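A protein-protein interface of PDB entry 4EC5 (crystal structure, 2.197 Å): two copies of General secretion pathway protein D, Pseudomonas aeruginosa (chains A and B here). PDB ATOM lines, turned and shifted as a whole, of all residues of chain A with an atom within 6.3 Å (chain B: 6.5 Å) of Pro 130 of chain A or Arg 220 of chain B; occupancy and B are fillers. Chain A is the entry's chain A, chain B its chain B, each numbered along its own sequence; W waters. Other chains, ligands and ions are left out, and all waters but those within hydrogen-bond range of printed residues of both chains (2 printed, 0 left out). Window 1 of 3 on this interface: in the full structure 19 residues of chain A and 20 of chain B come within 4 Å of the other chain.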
ATOM      1  N   VAL A 125     -13.019   5.016 -22.090  1.00  0.00           N
ATOM      2  CA  VAL A 125     -14.286   4.961 -22.825  1.00  0.00           C
ATOM      3  C   VAL A 125     -15.413   4.215 -22.107  1.00  0.00           C
ATOM      4  O   VAL A 125     -16.574   4.623 -22.167  1.00  0.00           O
ATOM      5  CB  VAL A 125     -14.169   4.469 -24.295  1.00  0.00           C
ATOM      6  CG1 VAL A 125     -13.626   5.568 -25.183  1.00  0.00           C
ATOM      7  CG2 VAL A 125     -13.312   3.214 -24.388  1.00  0.00           C
ATOM      8  N   SER A 126     -15.064   3.125 -21.434  1.00  0.00           N
ATOM      9  CA  SER A 126     -16.042   2.321 -20.709  1.00  0.00           C
ATOM     10  C   SER A 126     -16.873   3.120 -19.702  1.00  0.00           C
ATOM     11  O   SER A 126     -18.043   2.807 -19.480  1.00  0.00           O
ATOM     12  CB  SER A 126     -15.349   1.161 -19.990  1.00  0.00           C
ATOM     13  OG  SER A 126     -14.405   1.630 -19.044  1.00  0.00           O
ATOM     14  N   GLU A 127     -16.280   4.140 -19.091  1.00  0.00           N
ATOM     15  CA  GLU A 127     -17.004   4.957 -18.117  1.00  0.00           C
ATOM     16  C   GLU A 127     -18.039   5.896 -18.738  1.00  0.00           C
ATOM     17  O   GLU A 127     -18.983   6.316 -18.064  1.00  0.00           O
ATOM     18  CB  GLU A 127     -16.021   5.739 -17.237  1.00  0.00           C
ATOM     19  CG  GLU A 127     -15.147   4.862 -16.361  1.00  0.00           C
ATOM     20  CD  GLU A 127     -14.093   5.647 -15.605  1.00  0.00           C
ATOM     21  OE1 GLU A 127     -14.065   6.891 -15.727  1.00  0.00           O
ATOM     22  OE2 GLU A 127     -13.290   5.018 -14.883  1.00  0.00           O
ATOM     23  N   LEU A 128     -17.873   6.229 -20.013  1.00  0.00           N
ATOM     24  CA  LEU A 128     -18.816   7.113 -20.696  1.00  0.00           C
ATOM     25  C   LEU A 128     -20.013   6.380 -21.309  1.00  0.00           C
ATOM     26  O   LEU A 128     -21.078   6.970 -21.481  1.00  0.00           O
ATOM     27  CB  LEU A 128     -18.097   7.921 -21.782  1.00  0.00           C
ATOM     28  CG  LEU A 128     -16.899   8.734 -21.273  1.00  0.00           C
ATOM     29  CD1 LEU A 128     -16.195   9.468 -22.411  1.00  0.00           C
ATOM     30  CD2 LEU A 128     -17.326   9.703 -20.178  1.00  0.00           C
ATOM     31  N   ILE A 129     -19.837   5.103 -21.632  1.00  0.00           N
ATOM     32  CA  ILE A 129     -20.882   4.313 -22.293  1.00  0.00           C
ATOM     33  C   ILE A 129     -22.292   4.406 -21.692  1.00  0.00           C
ATOM     34  O   ILE A 129     -23.246   4.713 -22.407  1.00  0.00           O
ATOM     35  CB  ILE A 129     -20.467   2.824 -22.402  1.00  0.00           C
ATOM     36  CG1 ILE A 129     -19.282   2.665 -23.360  1.00  0.00           C
ATOM     37  CG2 ILE A 129     -21.678   1.960 -22.782  1.00  0.00           C
ATOM     38  CD1 ILE A 129     -19.656   2.266 -24.765  1.00  0.00           C
ATOM     39  N   PRO A 130     -22.435   4.143 -20.381  1.00  0.00           N
ATOM     40  CA  PRO A 130     -23.770   4.229 -19.767  1.00  0.00           C
ATOM     41  C   PRO A 130     -24.376   5.633 -19.723  1.00  0.00           C
ATOM     42  O   PRO A 130     -25.588   5.769 -19.576  1.00  0.00           O
ATOM     43  CB  PRO A 130     -23.584   3.637 -18.363  1.00  0.00           C
ATOM     44  CG  PRO A 130     -22.147   3.293 -18.221  1.00  0.00           C
ATOM     45  CD  PRO A 130     -21.386   3.812 -19.401  1.00  0.00           C
ATOM     46  N   LEU A 131     -23.540   6.657 -19.838  1.00  0.00           N
ATOM     47  CA  LEU A 131     -24.010   8.040 -19.811  1.00  0.00           C
ATOM     48  C   LEU A 131     -24.498   8.504 -21.183  1.00  0.00           C
ATOM     49  O   LEU A 131     -25.272   9.453 -21.281  1.00  0.00           O
ATOM     50  CB  LEU A 131     -22.889   8.954 -19.307  1.00  0.00           C
ATOM     51  CG  LEU A 131     -22.167   8.484 -18.040  1.00  0.00           C
ATOM     52  CD1 LEU A 131     -21.103   9.483 -17.618  1.00  0.00           C
ATOM     53  CD2 LEU A 131     -23.169   8.294 -16.915  1.00  0.00           C
ATOM     54  N   ILE A 132     -24.047   7.834 -22.241  1.00  0.00           N
ATOM     55  CA  ILE A 132     -24.454   8.193 -23.602  1.00  0.00           C
ATOM     56  C   ILE A 132     -25.483   7.236 -24.206  1.00  0.00           C
ATOM     57  O   ILE A 132     -26.149   7.584 -25.182  1.00  0.00           O
ATOM     58  CB  ILE A 132     -23.255   8.397 -24.553  1.00  0.00           C
ATOM     59  CG1 ILE A 132     -22.411   7.128 -24.644  1.00  0.00           C
ATOM     60  CG2 ILE A 132     -22.421   9.591 -24.108  1.00  0.00           C
ATOM     61  CD1 ILE A 132     -21.489   7.113 -25.841  1.00  0.00           C
ATOM     62  N   ARG A 133     -25.701   6.100 -23.562  1.00  0.00           N
ATOM     63  CA  ARG A 133     -26.631   5.118 -24.084  1.00  0.00           C
ATOM     64  C   ARG A 133     -28.004   5.724 -24.215  1.00  0.00           C
ATOM     65  O   ARG A 133     -28.685   5.483 -25.185  1.00  0.00           O
ATOM     66  CB  ARG A 133     -26.748   3.909 -23.170  1.00  0.00           C
ATOM     67  CG  ARG A 133     -25.811   2.790 -23.500  1.00  0.00           C
ATOM     68  CD  ARG A 133     -26.448   1.459 -23.244  1.00  0.00           C
ATOM     69  NE  ARG A 133     -25.450   0.477 -22.863  1.00  0.00           N
ATOM     70  CZ  ARG A 133     -24.734  -0.213 -23.739  1.00  0.00           C
ATOM     71  NH1 ARG A 133     -24.920  -0.024 -25.037  1.00  0.00           N
ATOM     72  NH2 ARG A 133     -23.838  -1.089 -23.321  1.00  0.00           N
ATOM     73  N   PRO A 134     -28.422   6.517 -23.248  1.00  0.00           N
ATOM     74  CA  PRO A 134     -29.748   7.140 -23.395  1.00  0.00           C
ATOM     75  C   PRO A 134     -29.934   7.973 -24.677  1.00  0.00           C
ATOM     76  O   PRO A 134     -31.076   8.279 -25.022  1.00  0.00           O
ATOM     77  CB  PRO A 134     -29.885   8.029 -22.153  1.00  0.00           C
ATOM     78  CG  PRO A 134     -28.762   7.694 -21.252  1.00  0.00           C
ATOM     79  CD  PRO A 134     -27.758   6.863 -21.977  1.00  0.00           C
ATOM     80  N   LEU A 142     -23.815   0.998 -30.432  1.00  0.00           N
ATOM     81  CA  LEU A 142     -22.792   1.582 -29.583  1.00  0.00           C
ATOM     82  C   LEU A 142     -21.846   0.479 -29.124  1.00  0.00           C
ATOM     83  O   LEU A 142     -22.278  -0.495 -28.506  1.00  0.00           O
ATOM     84  CB  LEU A 142     -23.421   2.315 -28.393  1.00  0.00           C
ATOM     85  CG  LEU A 142     -22.478   2.959 -27.378  1.00  0.00           C
ATOM     86  CD1 LEU A 142     -21.676   4.056 -28.059  1.00  0.00           C
ATOM     87  CD2 LEU A 142     -23.255   3.507 -26.188  1.00  0.00           C
ATOM     88  N   TYR A 178     -22.336   7.854 -10.856  1.00  0.00           N
ATOM     89  CA  TYR A 178     -23.688   8.346 -11.071  1.00  0.00           C
ATOM     90  C   TYR A 178     -24.717   7.585 -10.261  1.00  0.00           C
ATOM     91  O   TYR A 178     -24.495   6.443  -9.856  1.00  0.00           O
ATOM     92  CB  TYR A 178     -24.049   8.269 -12.560  1.00  0.00           C
ATOM     93  CG  TYR A 178     -24.003   6.882 -13.174  1.00  0.00           C
ATOM     94  CD1 TYR A 178     -22.844   6.382 -13.752  1.00  0.00           C
ATOM     95  CD2 TYR A 178     -25.142   6.087 -13.202  1.00  0.00           C
ATOM     96  CE1 TYR A 178     -22.816   5.122 -14.327  1.00  0.00           C
ATOM     97  CE2 TYR A 178     -25.125   4.826 -13.768  1.00  0.00           C
ATOM     98  CZ  TYR A 178     -23.960   4.349 -14.327  1.00  0.00           C
ATOM     99  OH  TYR A 178     -23.937   3.095 -14.893  1.00  0.00           O
ATOM    100  N   ARG A 220     -36.425   7.623 -16.234  1.00  0.00           N
ATOM    101  CA  ARG A 220     -35.492   7.741 -15.129  1.00  0.00           C
ATOM    102  C   ARG A 220     -34.440   8.819 -15.368  1.00  0.00           C
ATOM    103  O   ARG A 220     -34.146   9.178 -16.506  1.00  0.00           O
ATOM    104  CB  ARG A 220     -34.855   6.375 -14.875  1.00  0.00           C
ATOM    105  CG  ARG A 220     -33.832   5.988 -15.920  1.00  0.00           C
ATOM    106  CD  ARG A 220     -33.284   4.590 -15.706  1.00  0.00           C
ATOM    107  NE  ARG A 220     -32.176   4.340 -16.618  1.00  0.00           N
ATOM    108  CZ  ARG A 220     -31.261   3.389 -16.463  1.00  0.00           C
ATOM    109  NH1 ARG A 220     -30.294   3.261 -17.365  1.00  0.00           N
ATOM    110  NH2 ARG A 220     -31.319   2.554 -15.434  1.00  0.00           N
ATOM    111  N   ILE A 222     -30.449  10.171 -14.629  1.00  0.00           N
ATOM    112  CA  ILE A 222     -29.100   9.770 -14.275  1.00  0.00           C
ATOM    113  C   ILE A 222     -28.408  11.003 -13.737  1.00  0.00           C
ATOM    114  O   ILE A 222     -28.234  11.990 -14.455  1.00  0.00           O
ATOM    115  CB  ILE A 222     -28.328   9.208 -15.490  1.00  0.00           C
ATOM    116  CG1 ILE A 222     -28.961   7.913 -16.000  1.00  0.00           C
ATOM    117  CG2 ILE A 222     -26.868   8.957 -15.132  1.00  0.00           C
ATOM    118  CD1 ILE A 222     -28.563   7.575 -17.430  1.00  0.00           C
ATOM    119  N   PRO B 130     -29.487  -5.585 -16.699  1.00  0.00           N
ATOM    120  CA  PRO B 130     -28.268  -4.778 -16.561  1.00  0.00           C
ATOM    121  C   PRO B 130     -27.576  -4.955 -15.212  1.00  0.00           C
ATOM    122  O   PRO B 130     -26.362  -4.780 -15.122  1.00  0.00           O
ATOM    123  CB  PRO B 130     -28.771  -3.333 -16.707  1.00  0.00           C
ATOM    124  CG  PRO B 130     -30.111  -3.438 -17.338  1.00  0.00           C
ATOM    125  CD  PRO B 130     -30.679  -4.753 -16.939  1.00  0.00           C
ATOM    126  N   PRO B 134     -23.103  -7.788 -15.052  1.00  0.00           N
ATOM    127  CA  PRO B 134     -21.757  -7.716 -14.482  1.00  0.00           C
ATOM    128  C   PRO B 134     -21.274  -9.052 -13.915  1.00  0.00           C
ATOM    129  O   PRO B 134     -20.073  -9.316 -13.936  1.00  0.00           O
ATOM    130  CB  PRO B 134     -21.918  -6.695 -13.353  1.00  0.00           C
ATOM    131  CG  PRO B 134     -23.031  -5.804 -13.829  1.00  0.00           C
ATOM    132  CD  PRO B 134     -23.985  -6.728 -14.532  1.00  0.00           C
ATOM    133  N   VAL B 180     -23.668   4.076  -8.747  1.00  0.00           N
ATOM    134  CA  VAL B 180     -22.490   3.442  -9.332  1.00  0.00           C
ATOM    135  C   VAL B 180     -21.205   4.159  -8.921  1.00  0.00           C
ATOM    136  O   VAL B 180     -21.112   5.383  -9.000  1.00  0.00           O
ATOM    137  CB  VAL B 180     -22.616   3.372 -10.871  1.00  0.00           C
ATOM    138  CG1 VAL B 180     -21.314   2.894 -11.501  1.00  0.00           C
ATOM    139  CG2 VAL B 180     -23.788   2.475 -11.263  1.00  0.00           C
ATOM    140  N   ILE B 181     -20.220   3.388  -8.469  1.00  0.00           N
ATOM    141  CA  ILE B 181     -18.934   3.935  -8.064  1.00  0.00           C
ATOM    142  C   ILE B 181     -17.799   3.289  -8.856  1.00  0.00           C
ATOM    143  O   ILE B 181     -17.561   2.087  -8.741  1.00  0.00           O
ATOM    144  CB  ILE B 181     -18.657   3.735  -6.549  1.00  0.00           C
ATOM    145  CG1 ILE B 181     -19.797   4.285  -5.679  1.00  0.00           C
ATOM    146  CG2 ILE B 181     -17.294   4.333  -6.175  1.00  0.00           C
ATOM    147  CD1 ILE B 181     -19.999   5.777  -5.755  1.00  0.00           C
ATOM    148  N   ASN B 182     -17.103   4.096  -9.654  1.00  0.00           N
ATOM    149  CA  ASN B 182     -15.943   3.632 -10.404  1.00  0.00           C
ATOM    150  C   ASN B 182     -14.749   3.784  -9.475  1.00  0.00           C
ATOM    151  O   ASN B 182     -14.316   4.899  -9.189  1.00  0.00           O
ATOM    152  CB  ASN B 182     -15.704   4.473 -11.662  1.00  0.00           C
ATOM    153  CG  ASN B 182     -16.881   4.458 -12.624  1.00  0.00           C
ATOM    154  OD1 ASN B 182     -17.063   3.507 -13.384  1.00  0.00           O
ATOM    155  ND2 ASN B 182     -17.645   5.544 -12.642  1.00  0.00           N
ATOM    156  N   LEU B 183     -14.226   2.662  -8.994  1.00  0.00           N
ATOM    157  CA  LEU B 183     -13.158   2.692  -8.001  1.00  0.00           C
ATOM    158  C   LEU B 183     -11.849   3.161  -8.619  1.00  0.00           C
ATOM    159  O   LEU B 183     -11.529   2.837  -9.760  1.00  0.00           O
ATOM    160  CB  LEU B 183     -12.974   1.319  -7.336  1.00  0.00           C
ATOM    161  CG  LEU B 183     -14.097   0.758  -6.454  1.00  0.00           C
ATOM    162  CD1 LEU B 183     -13.688  -0.604  -5.897  1.00  0.00           C
ATOM    163  CD2 LEU B 183     -14.467   1.703  -5.326  1.00  0.00           C
ATOM    164  N   VAL B 188     -12.867  -4.103  -6.721  1.00  0.00           N
ATOM    165  CA  VAL B 188     -14.283  -4.356  -6.418  1.00  0.00           C
ATOM    166  C   VAL B 188     -14.597  -5.694  -5.740  1.00  0.00           C
ATOM    167  O   VAL B 188     -15.477  -5.741  -4.881  1.00  0.00           O
ATOM    168  CB  VAL B 188     -15.219  -4.179  -7.643  1.00  0.00           C
ATOM    169  CG1 VAL B 188     -15.289  -2.719  -8.058  1.00  0.00           C
ATOM    170  CG2 VAL B 188     -14.819  -5.094  -8.794  1.00  0.00           C
ATOM    171  N   ILE B 213     -23.337  -5.087  -5.823  1.00  0.00           N
ATOM    172  CA  ILE B 213     -23.017  -5.958  -6.935  1.00  0.00           C
ATOM    173  C   ILE B 213     -21.691  -5.467  -7.516  1.00  0.00           C
ATOM    174  O   ILE B 213     -21.593  -4.332  -7.981  1.00  0.00           O
ATOM    175  CB  ILE B 213     -24.125  -5.949  -7.996  1.00  0.00           C
ATOM    176  CG1 ILE B 213     -25.383  -6.637  -7.450  1.00  0.00           C
ATOM    177  CG2 ILE B 213     -23.630  -6.592  -9.286  1.00  0.00           C
ATOM    178  CD1 ILE B 213     -26.602  -6.472  -8.328  1.00  0.00           C
ATOM    179  N   ALA B 214     -20.677  -6.324  -7.488  1.00  0.00           N
ATOM    180  CA  ALA B 214     -19.364  -5.989  -8.025  1.00  0.00           C
ATOM    181  C   ALA B 214     -19.280  -6.225  -9.527  1.00  0.00           C
ATOM    182  O   ALA B 214     -19.664  -7.280 -10.022  1.00  0.00           O
ATOM    183  CB  ALA B 214     -18.311  -6.838  -7.338  1.00  0.00           C
ATOM    184  N   ASP B 215     -18.769  -5.228 -10.243  1.00  0.00           N
ATOM    185  CA  ASP B 215     -18.622  -5.309 -11.694  1.00  0.00           C
ATOM    186  C   ASP B 215     -17.132  -5.267 -12.013  1.00  0.00           C
ATOM    187  O   ASP B 215     -16.548  -4.214 -12.267  1.00  0.00           O
ATOM    188  CB  ASP B 215     -19.406  -4.186 -12.373  1.00  0.00           C
ATOM    189  CG  ASP B 215     -19.288  -4.221 -13.887  1.00  0.00           C
ATOM    190  OD1 ASP B 215     -18.666  -5.168 -14.414  1.00  0.00           O
ATOM    191  OD2 ASP B 215     -19.819  -3.302 -14.548  1.00  0.00           O
ATOM    192  N   ALA B 216     -16.545  -6.460 -11.995  1.00  0.00           N
ATOM    193  CA  ALA B 216     -15.114  -6.674 -12.160  1.00  0.00           C
ATOM    194  C   ALA B 216     -14.524  -6.250 -13.501  1.00  0.00           C
ATOM    195  O   ALA B 216     -13.359  -5.863 -13.565  1.00  0.00           O
ATOM    196  CB  ALA B 216     -14.781  -8.136 -11.898  1.00  0.00           C
ATOM    197  N   ARG B 217     -15.311  -6.322 -14.569  1.00  0.00           N
ATOM    198  CA  ARG B 217     -14.815  -5.904 -15.877  1.00  0.00           C
ATOM    199  C   ARG B 217     -14.369  -4.439 -15.907  1.00  0.00           C
ATOM    200  O   ARG B 217     -13.377  -4.103 -16.552  1.00  0.00           O
ATOM    201  CB  ARG B 217     -15.820  -6.202 -16.999  1.00  0.00           C
ATOM    202  CG  ARG B 217     -15.802  -7.649 -17.490  1.00  0.00           C
ATOM    203  CD  ARG B 217     -16.692  -7.846 -18.712  1.00  0.00           C
ATOM    204  NE  ARG B 217     -18.117  -7.676 -18.425  1.00  0.00           N
ATOM    205  CZ  ARG B 217     -18.915  -8.630 -17.950  1.00  0.00           C
ATOM    206  NH1 ARG B 217     -18.445  -9.846 -17.696  1.00  0.00           N
ATOM    207  NH2 ARG B 217     -20.196  -8.366 -17.723  1.00  0.00           N
ATOM    208  N   THR B 218     -15.101  -3.574 -15.211  1.00  0.00           N
ATOM    209  CA  THR B 218     -14.774  -2.149 -15.183  1.00  0.00           C
ATOM    210  C   THR B 218     -14.426  -1.644 -13.778  1.00  0.00           C
ATOM    211  O   THR B 218     -14.362  -0.434 -13.550  1.00  0.00           O
ATOM    212  CB  THR B 218     -15.902  -1.313 -15.822  1.00  0.00           C
ATOM    213  OG1 THR B 218     -17.148  -1.611 -15.182  1.00  0.00           O
ATOM    214  CG2 THR B 218     -16.010  -1.612 -17.314  1.00  0.00           C
ATOM    215  N   ASN B 219     -14.209  -2.567 -12.843  1.00  0.00           N
ATOM    216  CA  ASN B 219     -13.822  -2.207 -11.480  1.00  0.00           C
ATOM    217  C   ASN B 219     -14.741  -1.154 -10.860  1.00  0.00           C
ATOM    218  O   ASN B 219     -14.283  -0.109 -10.401  1.00  0.00           O
ATOM    219  CB  ASN B 219     -12.357  -1.759 -11.425  1.00  0.00           C
ATOM    220  CG  ASN B 219     -11.774  -1.844 -10.028  1.00  0.00           C
ATOM    221  OD1 ASN B 219     -12.076  -2.764  -9.273  1.00  0.00           O
ATOM    222  ND2 ASN B 219     -10.935  -0.876  -9.676  1.00  0.00           N
ATOM    223  N   ARG B 220     -16.037  -1.436 -10.861  1.00  0.00           N
ATOM    224  CA  ARG B 220     -17.028  -0.530 -10.290  1.00  0.00           C
ATOM    225  C   ARG B 220     -18.056  -1.273  -9.438  1.00  0.00           C
ATOM    226  O   ARG B 220     -18.321  -2.457  -9.654  1.00  0.00           O
ATOM    227  CB  ARG B 220     -17.698   0.267 -11.408  1.00  0.00           C
ATOM    228  CG  ARG B 220     -18.672  -0.569 -12.212  1.00  0.00           C
ATOM    229  CD  ARG B 220     -19.293   0.195 -13.367  1.00  0.00           C
ATOM    230  NE  ARG B 220     -20.359  -0.593 -13.982  1.00  0.00           N
ATOM    231  CZ  ARG B 220     -21.342  -0.101 -14.728  1.00  0.00           C
ATOM    232  NH1 ARG B 220     -22.251  -0.928 -15.230  1.00  0.00           N
ATOM    233  NH2 ARG B 220     -21.410   1.195 -14.999  1.00  0.00           N
ATOM    234  N   LEU B 221     -18.637  -0.559  -8.481  1.00  0.00           N
ATOM    235  CA  LEU B 221     -19.653  -1.110  -7.594  1.00  0.00           C
ATOM    236  C   LEU B 221     -21.034  -0.568  -7.939  1.00  0.00           C
ATOM    237  O   LEU B 221     -21.186   0.598  -8.308  1.00  0.00           O
ATOM    238  CB  LEU B 221     -19.358  -0.716  -6.148  1.00  0.00           C
ATOM    239  CG  LEU B 221     -18.023  -1.194  -5.578  1.00  0.00           C
ATOM    240  CD1 LEU B 221     -17.827  -0.673  -4.164  1.00  0.00           C
ATOM    241  CD2 LEU B 221     -17.954  -2.714  -5.599  1.00  0.00           C
ATOM    242  N   ILE B 222     -22.025  -1.426  -7.813  1.00  0.00           N
ATOM    243  CA  ILE B 222     -23.402  -1.023  -7.952  1.00  0.00           C
ATOM    244  C   ILE B 222     -24.068  -1.175  -6.589  1.00  0.00           C
ATOM    245  O   ILE B 222     -24.098  -2.260  -6.033  1.00  0.00           O
ATOM    246  CB  ILE B 222     -24.118  -1.869  -8.997  1.00  0.00           C
ATOM    247  CG1 ILE B 222     -23.391  -1.762 -10.328  1.00  0.00           C
ATOM    248  CG2 ILE B 222     -25.549  -1.426  -9.155  1.00  0.00           C
ATOM    249  CD1 ILE B 222     -23.750  -2.813 -11.310  1.00  0.00           C
HETATM  250  O   HOH W   1     -19.501   5.819 -15.371  1.00  0.00           O
HETATM  251  O   HOH W   2     -23.108   7.132  -7.090  1.00  0.00           O
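Ser 126 of chain A touches Thr 218 of chain B (CB to CG2, 3.9 Å).
CG of Glu 127 of chain A touches OD1 of Asn 182 of chain B, 3.8 Å away.
NH2 of Arg 220 of chain B touches CG of Pro 130 of chain A, at 3.9 Å.
Of chain B, only Arg 220 comes within 4 Å of Pro 130 of chain A.
Of the printed residues of chain B, Tyr 178 of chain A touches Val 180 and Arg 220.
Ile 222 of chain A touches none of the printed residues of chain B.
Printed residues of chain A within 4 Å of Val 180 of chain B: Tyr 178 (2.7 Å).
Ala 214 of chain B touches none of the printed residues of chain A.
The nearest residue of chain A that does not touch Arg 220 of chain B is Ser 126 of chain A (5.8 Å).
The nearest printed residue of chain A that does not touch Thr 218 of chain B is Glu 127 of chain A (5.7 Å).
The side-chain hydroxyl (OH) of Tyr 178 of chain A lies within hydrogen-bond range of the guanidinium group (NH2) of Arg 220 of chain B (3.2 Å).
The backbone NH (N) of Val 180 of chain B is in hydrogen-bond range of the backbone carbonyl oxygen (O) of Tyr 178 of chain A, 2.7 Å away.
Pro 130 of chain A touches Arg 220 of chain B, but with the chains exchanged Arg 220 of chain A does not touch Pro 130 of chain B (6.4 Å).
4 positions are printed for both chains.
Of the 5 pairs that touch across the chains among the printed residues, none has its exchanged pair printed and touching as well.
Hydrophobic or aromatic side chains of chain A that line the printed part of chain B: Pro 130 and Tyr 178.
Of the 17 printed residues of chain B, 4 touch a printed residue of chain A.
Hydrophobic or aromatic side chains of chain B that line the printed part of chain A: Val 180.
Among the printed residues, 5 pairs touch across the chains.
Among the printed residues, no Asp or Glu carboxylate lies within 4 Å of a Lys or Arg side-chain nitrogen of the other chain.
Water W1 bridges O of Glu 127 of chain A (2.8 Å) and ND2 of Asn 182 of chain B (3.3 Å).
Water W2 lies within hydrogen-bond range of the backbone carbonyl oxygen of Tyr 178 of chain A (3.2 Å) and the backbone carbonyl oxygen of Val 180 of chain B (3.3 Å).
OG1 of Thr 218 of chain B sits at hydrogen-bond distance from OD2 of Asp 215 of chain B, at 3.2 Å.
The side-chain carboxylate (OD2) of Asp 215 of chain B is in salt-bridge range of the guanidinium group (NE) of Arg 220 of chain B, at 2.8 Å.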
